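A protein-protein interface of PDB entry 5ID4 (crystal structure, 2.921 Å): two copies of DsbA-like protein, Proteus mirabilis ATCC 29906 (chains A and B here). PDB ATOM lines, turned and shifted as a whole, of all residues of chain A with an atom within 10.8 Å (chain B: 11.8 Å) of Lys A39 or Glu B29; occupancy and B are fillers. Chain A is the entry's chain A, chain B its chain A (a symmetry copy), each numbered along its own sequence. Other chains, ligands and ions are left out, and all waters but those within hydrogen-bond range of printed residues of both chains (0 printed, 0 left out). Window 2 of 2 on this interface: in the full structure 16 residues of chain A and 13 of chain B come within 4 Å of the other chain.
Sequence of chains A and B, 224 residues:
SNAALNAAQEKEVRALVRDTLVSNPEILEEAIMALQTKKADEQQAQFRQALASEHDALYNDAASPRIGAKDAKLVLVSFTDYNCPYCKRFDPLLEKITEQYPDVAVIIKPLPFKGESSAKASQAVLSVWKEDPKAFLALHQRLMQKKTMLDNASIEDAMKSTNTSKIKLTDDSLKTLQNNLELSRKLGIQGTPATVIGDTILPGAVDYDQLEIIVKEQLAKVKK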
ATOM      1  N   LEU A  28      20.681  12.942 -40.757  1.00  0.00           N
ATOM      2  CA  LEU A  28      21.410  13.519 -39.649  1.00  0.00           C
ATOM      3  C   LEU A  28      20.438  13.793 -38.520  1.00  0.00           C
ATOM      4  O   LEU A  28      20.749  13.580 -37.353  1.00  0.00           O
ATOM      5  CB  LEU A  28      22.118  14.788 -40.086  1.00  0.00           C
ATOM      6  CG  LEU A  28      22.992  15.470 -39.035  1.00  0.00           C
ATOM      7  CD1 LEU A  28      24.035  14.506 -38.490  1.00  0.00           C
ATOM      8  CD2 LEU A  28      23.653  16.737 -39.625  1.00  0.00           C
ATOM      9  N   ALA A  31      19.713  10.683 -36.711  1.00  0.00           N
ATOM     10  CA  ALA A  31      20.830  10.270 -35.892  1.00  0.00           C
ATOM     11  C   ALA A  31      20.872  11.113 -34.618  1.00  0.00           C
ATOM     12  O   ALA A  31      21.120  10.601 -33.521  1.00  0.00           O
ATOM     13  CB  ALA A  31      22.123  10.383 -36.663  1.00  0.00           C
ATOM     14  N   ILE A  32      20.620  12.406 -34.764  1.00  0.00           N
ATOM     15  CA  ILE A  32      20.506  13.270 -33.603  1.00  0.00           C
ATOM     16  C   ILE A  32      19.488  12.652 -32.650  1.00  0.00           C
ATOM     17  O   ILE A  32      19.834  12.163 -31.568  1.00  0.00           O
ATOM     18  CB  ILE A  32      20.078  14.687 -33.995  1.00  0.00           C
ATOM     19  CG1 ILE A  32      21.207  15.379 -34.746  1.00  0.00           C
ATOM     20  CG2 ILE A  32      19.701  15.515 -32.767  1.00  0.00           C
ATOM     21  CD1 ILE A  32      20.792  16.658 -35.392  1.00  0.00           C
ATOM     22  N   MET A  33      18.244  12.610 -33.106  1.00  0.00           N
ATOM     23  CA  MET A  33      17.143  12.089 -32.319  1.00  0.00           C
ATOM     24  C   MET A  33      17.503  10.808 -31.580  1.00  0.00           C
ATOM     25  O   MET A  33      17.122  10.618 -30.430  1.00  0.00           O
ATOM     26  CB  MET A  33      15.940  11.849 -33.228  1.00  0.00           C
ATOM     27  CG  MET A  33      15.258  13.134 -33.673  1.00  0.00           C
ATOM     28  SD  MET A  33      14.092  12.938 -35.060  1.00  0.00           S
ATOM     29  CE  MET A  33      13.071  11.573 -34.476  1.00  0.00           C
ATOM     30  N   ALA A  34      18.267   9.944 -32.233  1.00  0.00           N
ATOM     31  CA  ALA A  34      18.550   8.632 -31.685  1.00  0.00           C
ATOM     32  C   ALA A  34      19.649   8.724 -30.634  1.00  0.00           C
ATOM     33  O   ALA A  34      19.688   7.933 -29.696  1.00  0.00           O
ATOM     34  CB  ALA A  34      18.939   7.666 -32.804  1.00  0.00           C
ATOM     35  N   LEU A  35      20.532   9.701 -30.785  1.00  0.00           N
ATOM     36  CA  LEU A  35      21.557   9.950 -29.779  1.00  0.00           C
ATOM     37  C   LEU A  35      20.905  10.612 -28.551  1.00  0.00           C
ATOM     38  O   LEU A  35      21.171  10.229 -27.405  1.00  0.00           O
ATOM     39  CB  LEU A  35      22.672  10.827 -30.358  1.00  0.00           C
ATOM     40  CG  LEU A  35      23.742  11.324 -29.390  1.00  0.00           C
ATOM     41  CD1 LEU A  35      24.259  10.189 -28.549  1.00  0.00           C
ATOM     42  CD2 LEU A  35      24.882  11.988 -30.142  1.00  0.00           C
ATOM     43  N   GLN A  36      20.043  11.595 -28.802  1.00  0.00           N
ATOM     44  CA  GLN A  36      19.189  12.152 -27.765  1.00  0.00           C
ATOM     45  C   GLN A  36      18.426  11.072 -27.001  1.00  0.00           C
ATOM     46  O   GLN A  36      18.435  11.046 -25.766  1.00  0.00           O
ATOM     47  CB  GLN A  36      18.198  13.129 -28.376  1.00  0.00           C
ATOM     48  CG  GLN A  36      18.838  14.341 -29.010  1.00  0.00           C
ATOM     49  CD  GLN A  36      17.813  15.374 -29.454  1.00  0.00           C
ATOM     50  OE1 GLN A  36      16.629  15.067 -29.623  1.00  0.00           O
ATOM     51  NE2 GLN A  36      18.265  16.611 -29.637  1.00  0.00           N
ATOM     52  N   THR A  37      17.755  10.193 -27.737  1.00  0.00           N
ATOM     53  CA  THR A  37      16.937   9.165 -27.114  1.00  0.00           C
ATOM     54  C   THR A  37      17.807   8.247 -26.274  1.00  0.00           C
ATOM     55  O   THR A  37      17.384   7.771 -25.218  1.00  0.00           O
ATOM     56  CB  THR A  37      16.167   8.340 -28.153  1.00  0.00           C
ATOM     57  OG1 THR A  37      15.261   9.190 -28.863  1.00  0.00           O
ATOM     58  CG2 THR A  37      15.367   7.230 -27.487  1.00  0.00           C
ATOM     59  N   LYS A  38      19.028   8.008 -26.733  1.00  0.00           N
ATOM     60  CA  LYS A  38      19.957   7.183 -25.978  1.00  0.00           C
ATOM     61  C   LYS A  38      20.336   7.855 -24.653  1.00  0.00           C
ATOM     62  O   LYS A  38      20.291   7.228 -23.590  1.00  0.00           O
ATOM     63  CB  LYS A  38      21.204   6.903 -26.804  1.00  0.00           C
ATOM     64  CG  LYS A  38      22.242   6.045 -26.100  1.00  0.00           C
ATOM     65  CD  LYS A  38      23.283   5.561 -27.105  1.00  0.00           C
ATOM     66  CE  LYS A  38      24.367   4.710 -26.445  1.00  0.00           C
ATOM     67  NZ  LYS A  38      25.509   5.532 -25.960  1.00  0.00           N
ATOM     68  N   LYS A  39      20.689   9.133 -24.713  1.00  0.00           N
ATOM     69  CA  LYS A  39      21.132   9.850 -23.522  1.00  0.00           C
ATOM     70  C   LYS A  39      20.006  10.004 -22.495  1.00  0.00           C
ATOM     71  O   LYS A  39      20.220   9.824 -21.290  1.00  0.00           O
ATOM     72  CB  LYS A  39      21.685  11.212 -23.909  1.00  0.00           C
ATOM     73  CG  LYS A  39      23.128  11.177 -24.364  1.00  0.00           C
ATOM     74  CD  LYS A  39      23.536  12.528 -24.889  1.00  0.00           C
ATOM     75  CE  LYS A  39      24.990  12.579 -25.363  1.00  0.00           C
ATOM     76  NZ  LYS A  39      25.385  14.020 -25.701  1.00  0.00           N
ATOM     77  N   ALA A  40      18.814  10.338 -22.978  1.00  0.00           N
ATOM     78  CA  ALA A  40      17.630  10.409 -22.128  1.00  0.00           C
ATOM     79  C   ALA A  40      17.445   9.123 -21.349  1.00  0.00           C
ATOM     80  O   ALA A  40      17.504   9.108 -20.127  1.00  0.00           O
ATOM     81  CB  ALA A  40      16.411  10.679 -22.960  1.00  0.00           C
ATOM     82  N   ASP A  41      17.224   8.047 -22.087  1.00  0.00           N
ATOM     83  CA  ASP A  41      17.057   6.723 -21.516  1.00  0.00           C
ATOM     84  C   ASP A  41      18.145   6.394 -20.494  1.00  0.00           C
ATOM     85  O   ASP A  41      17.870   5.772 -19.468  1.00  0.00           O
ATOM     86  CB  ASP A  41      17.049   5.665 -22.635  1.00  0.00           C
ATOM     87  CG  ASP A  41      15.791   5.731 -23.506  1.00  0.00           C
ATOM     88  OD1 ASP A  41      14.824   6.431 -23.128  1.00  0.00           O
ATOM     89  OD2 ASP A  41      15.765   5.068 -24.567  1.00  0.00           O
ATOM     90  N   GLU A  42      19.376   6.810 -20.763  1.00  0.00           N
ATOM     91  CA  GLU A  42      20.461   6.543 -19.830  1.00  0.00           C
ATOM     92  C   GLU A  42      20.215   7.272 -18.517  1.00  0.00           C
ATOM     93  O   GLU A  42      20.219   6.664 -17.443  1.00  0.00           O
ATOM     94  CB  GLU A  42      21.798   6.961 -20.427  1.00  0.00           C
ATOM     95  CG  GLU A  42      22.302   5.992 -21.481  1.00  0.00           C
ATOM     96  CD  GLU A  42      23.411   6.574 -22.342  1.00  0.00           C
ATOM     97  OE1 GLU A  42      24.012   5.805 -23.118  1.00  0.00           O
ATOM     98  OE2 GLU A  42      23.680   7.792 -22.251  1.00  0.00           O
ATOM     99  N   GLN A  43      19.989   8.576 -18.607  1.00  0.00           N
ATOM    100  CA  GLN A  43      19.697   9.370 -17.421  1.00  0.00           C
ATOM    101  C   GLN A  43      18.514   8.830 -16.637  1.00  0.00           C
ATOM    102  O   GLN A  43      18.593   8.690 -15.416  1.00  0.00           O
ATOM    103  CB  GLN A  43      19.412  10.813 -17.799  1.00  0.00           C
ATOM    104  CG  GLN A  43      20.646  11.607 -18.125  1.00  0.00           C
ATOM    105  CD  GLN A  43      20.405  13.097 -18.019  1.00  0.00           C
ATOM    106  OE1 GLN A  43      19.261  13.550 -17.867  1.00  0.00           O
ATOM    107  NE2 GLN A  43      21.480  13.875 -18.090  1.00  0.00           N
ATOM    108  N   GLN A  44      17.415   8.549 -17.332  1.00  0.00           N
ATOM    109  CA  GLN A  44      16.224   8.058 -16.664  1.00  0.00           C
ATOM    110  C   GLN A  44      16.587   6.833 -15.847  1.00  0.00           C
ATOM    111  O   GLN A  44      16.183   6.704 -14.703  1.00  0.00           O
ATOM    112  CB  GLN A  44      15.115   7.721 -17.655  1.00  0.00           C
ATOM    113  CG  GLN A  44      13.800   7.311 -16.972  1.00  0.00           C
ATOM    114  CD  GLN A  44      12.809   6.644 -17.926  1.00  0.00           C
ATOM    115  OE1 GLN A  44      12.806   6.920 -19.130  1.00  0.00           O
ATOM    116  NE2 GLN A  44      11.967   5.754 -17.387  1.00  0.00           N
ATOM    117  N   ALA A  45      17.381   5.946 -16.422  1.00  0.00           N
ATOM    118  CA  ALA A  45      17.789   4.754 -15.704  1.00  0.00           C
ATOM    119  C   ALA A  45      18.713   5.129 -14.562  1.00  0.00           C
ATOM    120  O   ALA A  45      18.708   4.490 -13.510  1.00  0.00           O
ATOM    121  CB  ALA A  45      18.467   3.791 -16.623  1.00  0.00           C
ATOM    122  N   GLN A  46      19.504   6.175 -14.771  1.00  0.00           N
ATOM    123  CA  GLN A  46      20.444   6.630 -13.753  1.00  0.00           C
ATOM    124  C   GLN A  46      19.734   7.261 -12.555  1.00  0.00           C
ATOM    125  O   GLN A  46      20.155   7.071 -11.410  1.00  0.00           O
ATOM    126  CB  GLN A  46      21.428   7.626 -14.347  1.00  0.00           C
ATOM    127  CG  GLN A  46      22.719   7.723 -13.558  1.00  0.00           C
ATOM    128  CD  GLN A  46      23.911   8.054 -14.442  1.00  0.00           C
ATOM    129  OE1 GLN A  46      23.814   8.894 -15.343  1.00  0.00           O
ATOM    130  NE2 GLN A  46      25.041   7.381 -14.198  1.00  0.00           N
ATOM    131  N   PHE A  47      18.670   8.014 -12.822  1.00  0.00           N
ATOM    132  CA  PHE A  47      17.821   8.511 -11.753  1.00  0.00           C
ATOM    133  C   PHE A  47      17.242   7.317 -11.034  1.00  0.00           C
ATOM    134  O   PHE A  47      17.418   7.174  -9.830  1.00  0.00           O
ATOM    135  CB  PHE A  47      16.699   9.416 -12.281  1.00  0.00           C
ATOM    136  CG  PHE A  47      17.110  10.863 -12.481  1.00  0.00           C
ATOM    137  CD1 PHE A  47      16.602  11.601 -13.548  1.00  0.00           C
ATOM    138  CD2 PHE A  47      17.989  11.493 -11.600  1.00  0.00           C
ATOM    139  CE1 PHE A  47      16.971  12.934 -13.742  1.00  0.00           C
ATOM    140  CE2 PHE A  47      18.365  12.823 -11.789  1.00  0.00           C
ATOM    141  CZ  PHE A  47      17.851  13.542 -12.859  1.00  0.00           C
ATOM    142  N   ARG A  48      16.586   6.437 -11.782  1.00  0.00           N
ATOM    143  CA  ARG A  48      15.870   5.316 -11.190  1.00  0.00           C
ATOM    144  C   ARG A  48      16.759   4.509 -10.246  1.00  0.00           C
ATOM    145  O   ARG A  48      16.257   3.814  -9.364  1.00  0.00           O
ATOM    146  CB  ARG A  48      15.299   4.406 -12.275  1.00  0.00           C
ATOM    147  CG  ARG A  48      14.165   5.025 -13.086  1.00  0.00           C
ATOM    148  CD  ARG A  48      13.200   3.972 -13.601  1.00  0.00           C
ATOM    149  NE  ARG A  48      12.409   3.389 -12.514  1.00  0.00           N
ATOM    150  CZ  ARG A  48      11.364   2.582 -12.694  1.00  0.00           C
ATOM    151  NH1 ARG A  48      10.984   2.267 -13.927  1.00  0.00           N
ATOM    152  NH2 ARG A  48      10.694   2.097 -11.647  1.00  0.00           N
ATOM    153  N   VAL B  17      24.969   3.973 -44.362  1.00  0.00           N
ATOM    154  CA  VAL B  17      25.236   5.221 -43.663  1.00  0.00           C
ATOM    155  C   VAL B  17      24.178   5.450 -42.562  1.00  0.00           C
ATOM    156  O   VAL B  17      24.462   5.508 -41.340  1.00  0.00           O
ATOM    157  CB  VAL B  17      25.217   6.408 -44.639  1.00  0.00           C
ATOM    158  CG1 VAL B  17      25.397   7.709 -43.901  1.00  0.00           C
ATOM    159  CG2 VAL B  17      26.297   6.279 -45.655  1.00  0.00           C
ATOM    160  N   THR B  20      24.062   2.879 -39.886  1.00  0.00           N
ATOM    161  CA  THR B  20      25.219   2.908 -38.999  1.00  0.00           C
ATOM    162  C   THR B  20      25.042   4.011 -37.965  1.00  0.00           C
ATOM    163  O   THR B  20      25.138   3.763 -36.761  1.00  0.00           O
ATOM    164  CB  THR B  20      26.553   3.138 -39.763  1.00  0.00           C
ATOM    165  OG1 THR B  20      26.531   2.437 -41.007  1.00  0.00           O
ATOM    166  CG2 THR B  20      27.727   2.643 -38.949  1.00  0.00           C
ATOM    167  N   LEU B  21      24.757   5.221 -38.431  1.00  0.00           N
ATOM    168  CA  LEU B  21      24.665   6.333 -37.501  1.00  0.00           C
ATOM    169  C   LEU B  21      23.461   6.195 -36.584  1.00  0.00           C
ATOM    170  O   LEU B  21      23.538   6.516 -35.398  1.00  0.00           O
ATOM    171  CB  LEU B  21      24.591   7.651 -38.250  1.00  0.00           C
ATOM    172  CG  LEU B  21      25.807   7.984 -39.106  1.00  0.00           C
ATOM    173  CD1 LEU B  21      25.542   9.291 -39.834  1.00  0.00           C
ATOM    174  CD2 LEU B  21      27.083   8.070 -38.282  1.00  0.00           C
ATOM    175  N   VAL B  22      22.348   5.730 -37.129  1.00  0.00           N
ATOM    176  CA  VAL B  22      21.129   5.657 -36.348  1.00  0.00           C
ATOM    177  C   VAL B  22      21.083   4.475 -35.386  1.00  0.00           C
ATOM    178  O   VAL B  22      20.536   4.597 -34.304  1.00  0.00           O
ATOM    179  CB  VAL B  22      19.915   5.613 -37.267  1.00  0.00           C
ATOM    180  CG1 VAL B  22      18.650   5.347 -36.492  1.00  0.00           C
ATOM    181  CG2 VAL B  22      19.804   6.918 -38.011  1.00  0.00           C
ATOM    182  N   SER B  23      21.639   3.334 -35.758  1.00  0.00           N
ATOM    183  CA  SER B  23      21.596   2.164 -34.890  1.00  0.00           C
ATOM    184  C   SER B  23      22.754   2.249 -33.928  1.00  0.00           C
ATOM    185  O   SER B  23      22.744   1.626 -32.871  1.00  0.00           O
ATOM    186  CB  SER B  23      21.654   0.866 -35.698  1.00  0.00           C
ATOM    187  OG  SER B  23      22.653   0.921 -36.714  1.00  0.00           O
ATOM    188  N   ASN B  24      23.752   3.039 -34.302  1.00  0.00           N
ATOM    189  CA  ASN B  24      24.854   3.336 -33.407  1.00  0.00           C
ATOM    190  C   ASN B  24      25.119   4.840 -33.326  1.00  0.00           C
ATOM    191  O   ASN B  24      25.944   5.391 -34.051  1.00  0.00           O
ATOM    192  CB  ASN B  24      26.110   2.600 -33.843  1.00  0.00           C
ATOM    193  CG  ASN B  24      27.213   2.669 -32.791  1.00  0.00           C
ATOM    194  OD1 ASN B  24      27.181   3.496 -31.848  1.00  0.00           O
ATOM    195  ND2 ASN B  24      28.202   1.789 -32.942  1.00  0.00           N
ATOM    196  N   PRO B  25      24.392   5.513 -32.437  1.00  0.00           N
ATOM    197  CA  PRO B  25      24.501   6.942 -32.146  1.00  0.00           C
ATOM    198  C   PRO B  25      25.909   7.400 -31.798  1.00  0.00           C
ATOM    199  O   PRO B  25      26.315   8.512 -32.166  1.00  0.00           O
ATOM    200  CB  PRO B  25      23.602   7.108 -30.935  1.00  0.00           C
ATOM    201  CG  PRO B  25      22.597   6.011 -31.076  1.00  0.00           C
ATOM    202  CD  PRO B  25      23.284   4.876 -31.711  1.00  0.00           C
ATOM    203  N   GLU B  26      26.651   6.550 -31.095  1.00  0.00           N
ATOM    204  CA  GLU B  26      27.940   6.952 -30.555  1.00  0.00           C
ATOM    205  C   GLU B  26      28.895   7.446 -31.625  1.00  0.00           C
ATOM    206  O   GLU B  26      29.786   8.238 -31.334  1.00  0.00           O
ATOM    207  CB  GLU B  26      28.590   5.806 -29.789  1.00  0.00           C
ATOM    208  CG  GLU B  26      28.007   5.618 -28.412  1.00  0.00           C
ATOM    209  CD  GLU B  26      28.080   6.892 -27.535  1.00  0.00           C
ATOM    210  OE1 GLU B  26      29.183   7.264 -27.038  1.00  0.00           O
ATOM    211  OE2 GLU B  26      27.013   7.528 -27.336  1.00  0.00           O
ATOM    212  N   ILE B  27      28.712   7.008 -32.865  1.00  0.00           N
ATOM    213  CA  ILE B  27      29.622   7.425 -33.926  1.00  0.00           C
ATOM    214  C   ILE B  27      29.410   8.902 -34.162  1.00  0.00           C
ATOM    215  O   ILE B  27      30.350   9.640 -34.446  1.00  0.00           O
ATOM    216  CB  ILE B  27      29.409   6.624 -35.237  1.00  0.00           C
ATOM    217  CG1 ILE B  27      29.769   5.162 -35.013  1.00  0.00           C
ATOM    218  CG2 ILE B  27      30.275   7.139 -36.365  1.00  0.00           C
ATOM    219  CD1 ILE B  27      28.590   4.262 -35.109  1.00  0.00           C
ATOM    220  N   LEU B  28      28.164   9.336 -34.005  1.00  0.00           N
ATOM    221  CA  LEU B  28      27.834  10.731 -34.198  1.00  0.00           C
ATOM    222  C   LEU B  28      28.469  11.538 -33.085  1.00  0.00           C
ATOM    223  O   LEU B  28      28.980  12.629 -33.307  1.00  0.00           O
ATOM    224  CB  LEU B  28      26.328  10.918 -34.223  1.00  0.00           C
ATOM    225  CG  LEU B  28      25.828  12.335 -34.494  1.00  0.00           C
ATOM    226  CD1 LEU B  28      26.397  12.870 -35.801  1.00  0.00           C
ATOM    227  CD2 LEU B  28      24.282  12.370 -34.501  1.00  0.00           C
ATOM    228  N   GLU B  29      28.470  10.979 -31.885  1.00  0.00           N
ATOM    229  CA  GLU B  29      29.100  11.659 -30.775  1.00  0.00           C
ATOM    230  C   GLU B  29      30.590  11.790 -31.012  1.00  0.00           C
ATOM    231  O   GLU B  29      31.176  12.822 -30.684  1.00  0.00           O
ATOM    232  CB  GLU B  29      28.845  10.933 -29.461  1.00  0.00           C
ATOM    233  CG  GLU B  29      29.284  11.721 -28.240  1.00  0.00           C
ATOM    234  CD  GLU B  29      28.653  11.174 -26.964  1.00  0.00           C
ATOM    235  OE1 GLU B  29      28.291   9.961 -26.996  1.00  0.00           O
ATOM    236  OE2 GLU B  29      28.506  11.944 -25.949  1.00  0.00           O
ATOM    237  N   GLU B  30      31.211  10.755 -31.576  1.00  0.00           N
ATOM    238  CA  GLU B  30      32.650  10.803 -31.837  1.00  0.00           C
ATOM    239  C   GLU B  30      32.965  11.862 -32.873  1.00  0.00           C
ATOM    240  O   GLU B  30      34.023  12.495 -32.841  1.00  0.00           O
ATOM    241  CB  GLU B  30      33.179   9.457 -32.315  1.00  0.00           C
ATOM    242  CG  GLU B  30      33.401   8.443 -31.198  1.00  0.00           C
ATOM    243  CD  GLU B  30      34.151   7.182 -31.673  1.00  0.00           C
ATOM    244  OE1 GLU B  30      35.397   7.137 -31.520  1.00  0.00           O
ATOM    245  OE2 GLU B  30      33.493   6.239 -32.188  1.00  0.00           O
ATOM    246  N   ALA B  31      32.032  12.057 -33.792  1.00  0.00           N
ATOM    247  CA  ALA B  31      32.232  13.022 -34.849  1.00  0.00           C
ATOM    248  C   ALA B  31      32.037  14.434 -34.300  1.00  0.00           C
ATOM    249  O   ALA B  31      32.791  15.357 -34.627  1.00  0.00           O
ATOM    250  CB  ALA B  31      31.290  12.749 -35.998  1.00  0.00           C
ATOM    251  N   ILE B  32      31.029  14.599 -33.454  1.00  0.00           N
ATOM    252  CA  ILE B  32      30.838  15.867 -32.774  1.00  0.00           C
ATOM    253  C   ILE B  32      32.148  16.242 -32.091  1.00  0.00           C
ATOM    254  O   ILE B  32      32.837  17.188 -32.494  1.00  0.00           O
ATOM    255  CB  ILE B  32      29.704  15.791 -31.747  1.00  0.00           C
ATOM    256  CG1 ILE B  32      28.368  15.656 -32.464  1.00  0.00           C
ATOM    257  CG2 ILE B  32      29.679  17.029 -30.853  1.00  0.00           C
ATOM    258  CD1 ILE B  32      27.239  15.313 -31.550  1.00  0.00           C
ATOM    259  N   MET B  33      32.520  15.437 -31.106  1.00  0.00           N
ATOM    260  CA  MET B  33      33.720  15.663 -30.324  1.00  0.00           C
ATOM    261  C   MET B  33      34.911  16.072 -31.180  1.00  0.00           C
ATOM    262  O   MET B  33      35.686  16.944 -30.802  1.00  0.00           O
ATOM    263  CB  MET B  33      34.053  14.401 -29.532  1.00  0.00           C
ATOM    264  CG  MET B  33      33.112  14.161 -28.360  1.00  0.00           C
ATOM    265  SD  MET B  33      33.203  12.491 -27.639  1.00  0.00           S
ATOM    266  CE  MET B  33      34.977  12.313 -27.374  1.00  0.00           C
ATOM    267  N   ALA B  34      35.035  15.464 -32.350  1.00  0.00           N
ATOM    268  CA  ALA B  34      36.205  15.667 -33.180  1.00  0.00           C
ATOM    269  C   ALA B  34      36.093  16.983 -33.940  1.00  0.00           C
ATOM    270  O   ALA B  34      37.097  17.617 -34.249  1.00  0.00           O
ATOM    271  CB  ALA B  34      36.382  14.491 -34.141  1.00  0.00           C
ATOM    272  N   LEU B  35      34.867  17.398 -34.225  1.00  0.00           N
ATOM    273  CA  LEU B  35      34.639  18.696 -34.848  1.00  0.00           C
ATOM    274  C   LEU B  35      34.864  19.802 -33.801  1.00  0.00           C
ATOM    275  O   LEU B  35      35.525  20.813 -34.073  1.00  0.00           O
ATOM    276  CB  LEU B  35      33.225  18.765 -35.437  1.00  0.00           C
ATOM    277  CG  LEU B  35      32.762  20.114 -35.979  1.00  0.00           C
ATOM    278  CD1 LEU B  35      33.808  20.707 -36.883  1.00  0.00           C
ATOM    279  CD2 LEU B  35      31.443  19.973 -36.719  1.00  0.00           C
ATOM    280  N   GLN B  36      34.321  19.596 -32.603  1.00  0.00           N
ATOM    281  CA  GLN B  36      34.639  20.437 -31.460  1.00  0.00           C
ATOM    282  C   GLN B  36      36.145  20.585 -31.251  1.00  0.00           C
ATOM    283  O   GLN B  36      36.658  21.700 -31.113  1.00  0.00           O
ATOM    284  CB  GLN B  36      34.012  19.863 -30.200  1.00  0.00           C
ATOM    285  CG  GLN B  36      32.503  19.834 -30.221  1.00  0.00           C
ATOM    286  CD  GLN B  36      31.910  19.417 -28.883  1.00  0.00           C
ATOM    287  OE1 GLN B  36      32.588  18.813 -28.046  1.00  0.00           O
ATOM    288  NE2 GLN B  36      30.640  19.747 -28.673  1.00  0.00           N
ATOM    289  N   THR B  37      36.848  19.457 -31.211  1.00  0.00           N
ATOM    290  CA  THR B  37      38.278  19.475 -30.946  1.00  0.00           C
ATOM    291  C   THR B  37      38.999  20.237 -32.044  1.00  0.00           C
ATOM    292  O   THR B  37      39.987  20.928 -31.785  1.00  0.00           O
ATOM    293  CB  THR B  37      38.855  18.058 -30.834  1.00  0.00           C
ATOM    294  OG1 THR B  37      38.256  17.384 -29.724  1.00  0.00           O
ATOM    295  CG2 THR B  37      40.361  18.097 -30.620  1.00  0.00           C
ATOM    296  N   LYS B  38      38.500  20.125 -33.266  1.00  0.00           N
ATOM    297  CA  LYS B  38      39.086  20.855 -34.379  1.00  0.00           C
ATOM    298  C   LYS B  38      38.912  22.366 -34.196  1.00  0.00           C
ATOM    299  O   LYS B  38      39.868  23.136 -34.336  1.00  0.00           O
ATOM    300  CB  LYS B  38      38.464  20.405 -35.692  1.00  0.00           C
ATOM    301  CG  LYS B  38      39.011  21.112 -36.920  1.00  0.00           C
ATOM    302  CD  LYS B  38      38.569  20.378 -38.183  1.00  0.00           C
ATOM    303  CE  LYS B  38      39.075  21.062 -39.453  1.00  0.00           C
ATOM    304  NZ  LYS B  38      38.121  22.088 -39.955  1.00  0.00           N
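Among the printed residues, merely in contact across the chains: Ala A31 with Leu B28 (3.6 Å), Ile A32 with Leu B28 (3.7 Å), Leu A35 with Pro B25 (3.7 Å), Ala A34 with Pro B25 (3.7 Å), Ala A34 with Val B22 (3.8 Å), Leu A28 with Leu B28 (3.9 Å) and Ala A31 with Val B22 (3.98 Å).
Leu B28 touches its own counterpart, Leu A28. Ala A31 touches Leu B28, but with the chains exchanged Leu A28 does not touch Ala B31 (7.9 Å). Ile A32 touches Leu B28, but with the chains exchanged Leu A28 does not touch Ile B32 (7.5 Å). 9 positions are printed for both chains.
Of the printed residues of chain B, Leu A28 touches Leu B28. Of the printed residues of chain B, Ala A34 touches Val B22 (3.8 Å) and Pro B25 (3.7 Å). Of chain B, only Glu B29 comes within 4 Å of Lys A39. No residue of chain B comes within 4 Å of Ala A40. No residue of chain B comes within 4 Å of Asp A41. No residue of chain B comes within 4 Å of Glu A42. No residue of chain B comes within 4 Å of Gln A43. Printed residues of chain A within 4 Å of Pro B25: Ala A34 (3.7 Å) and Leu A35 (3.7 Å). Of the printed residues of chain A, Glu B26 touches Lys A38 (2.9 Å). Of chain A, only Leu A28, Ala A31 and Ile A32 come within 4 Å of Leu B28. Glu B29 touches one residue of chain A. No residue of chain A comes within 4 Å of Glu B30. Ile B32 touches none of the printed residues of chain A. The nearest residue of chain B that does not touch Lys A39 is Glu B26 (5.8 Å). The nearest residue of chain A that does not touch Glu B29 is Leu A35 (4.1 Å). The nearest printed residue of chain B that does not touch Leu A28 is Leu B21 (5.6 Å).
NZ of Lys A38 is in salt-bridge range of OE2 of Glu B26 (2.9 Å). NZ of Lys A39 is in salt-bridge range of OE2 of Glu B29.
The side-chain amino group of Lys A38 lies within salt-bridge range of the side-chain carboxylate of Glu A42. The side-chain amide oxygen (OD1) of Asn B24 is in hydrogen-bond range of the backbone NH (N) of Glu B26.
Of the 19 printed residues of chain A, 7 touch a printed residue of chain B. Hydrophobic or aromatic side chains of chain B that line the printed part of chain A: Val B22, Pro B25 and Leu B28. Among the printed residues, 9 pairs touch across the chains.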
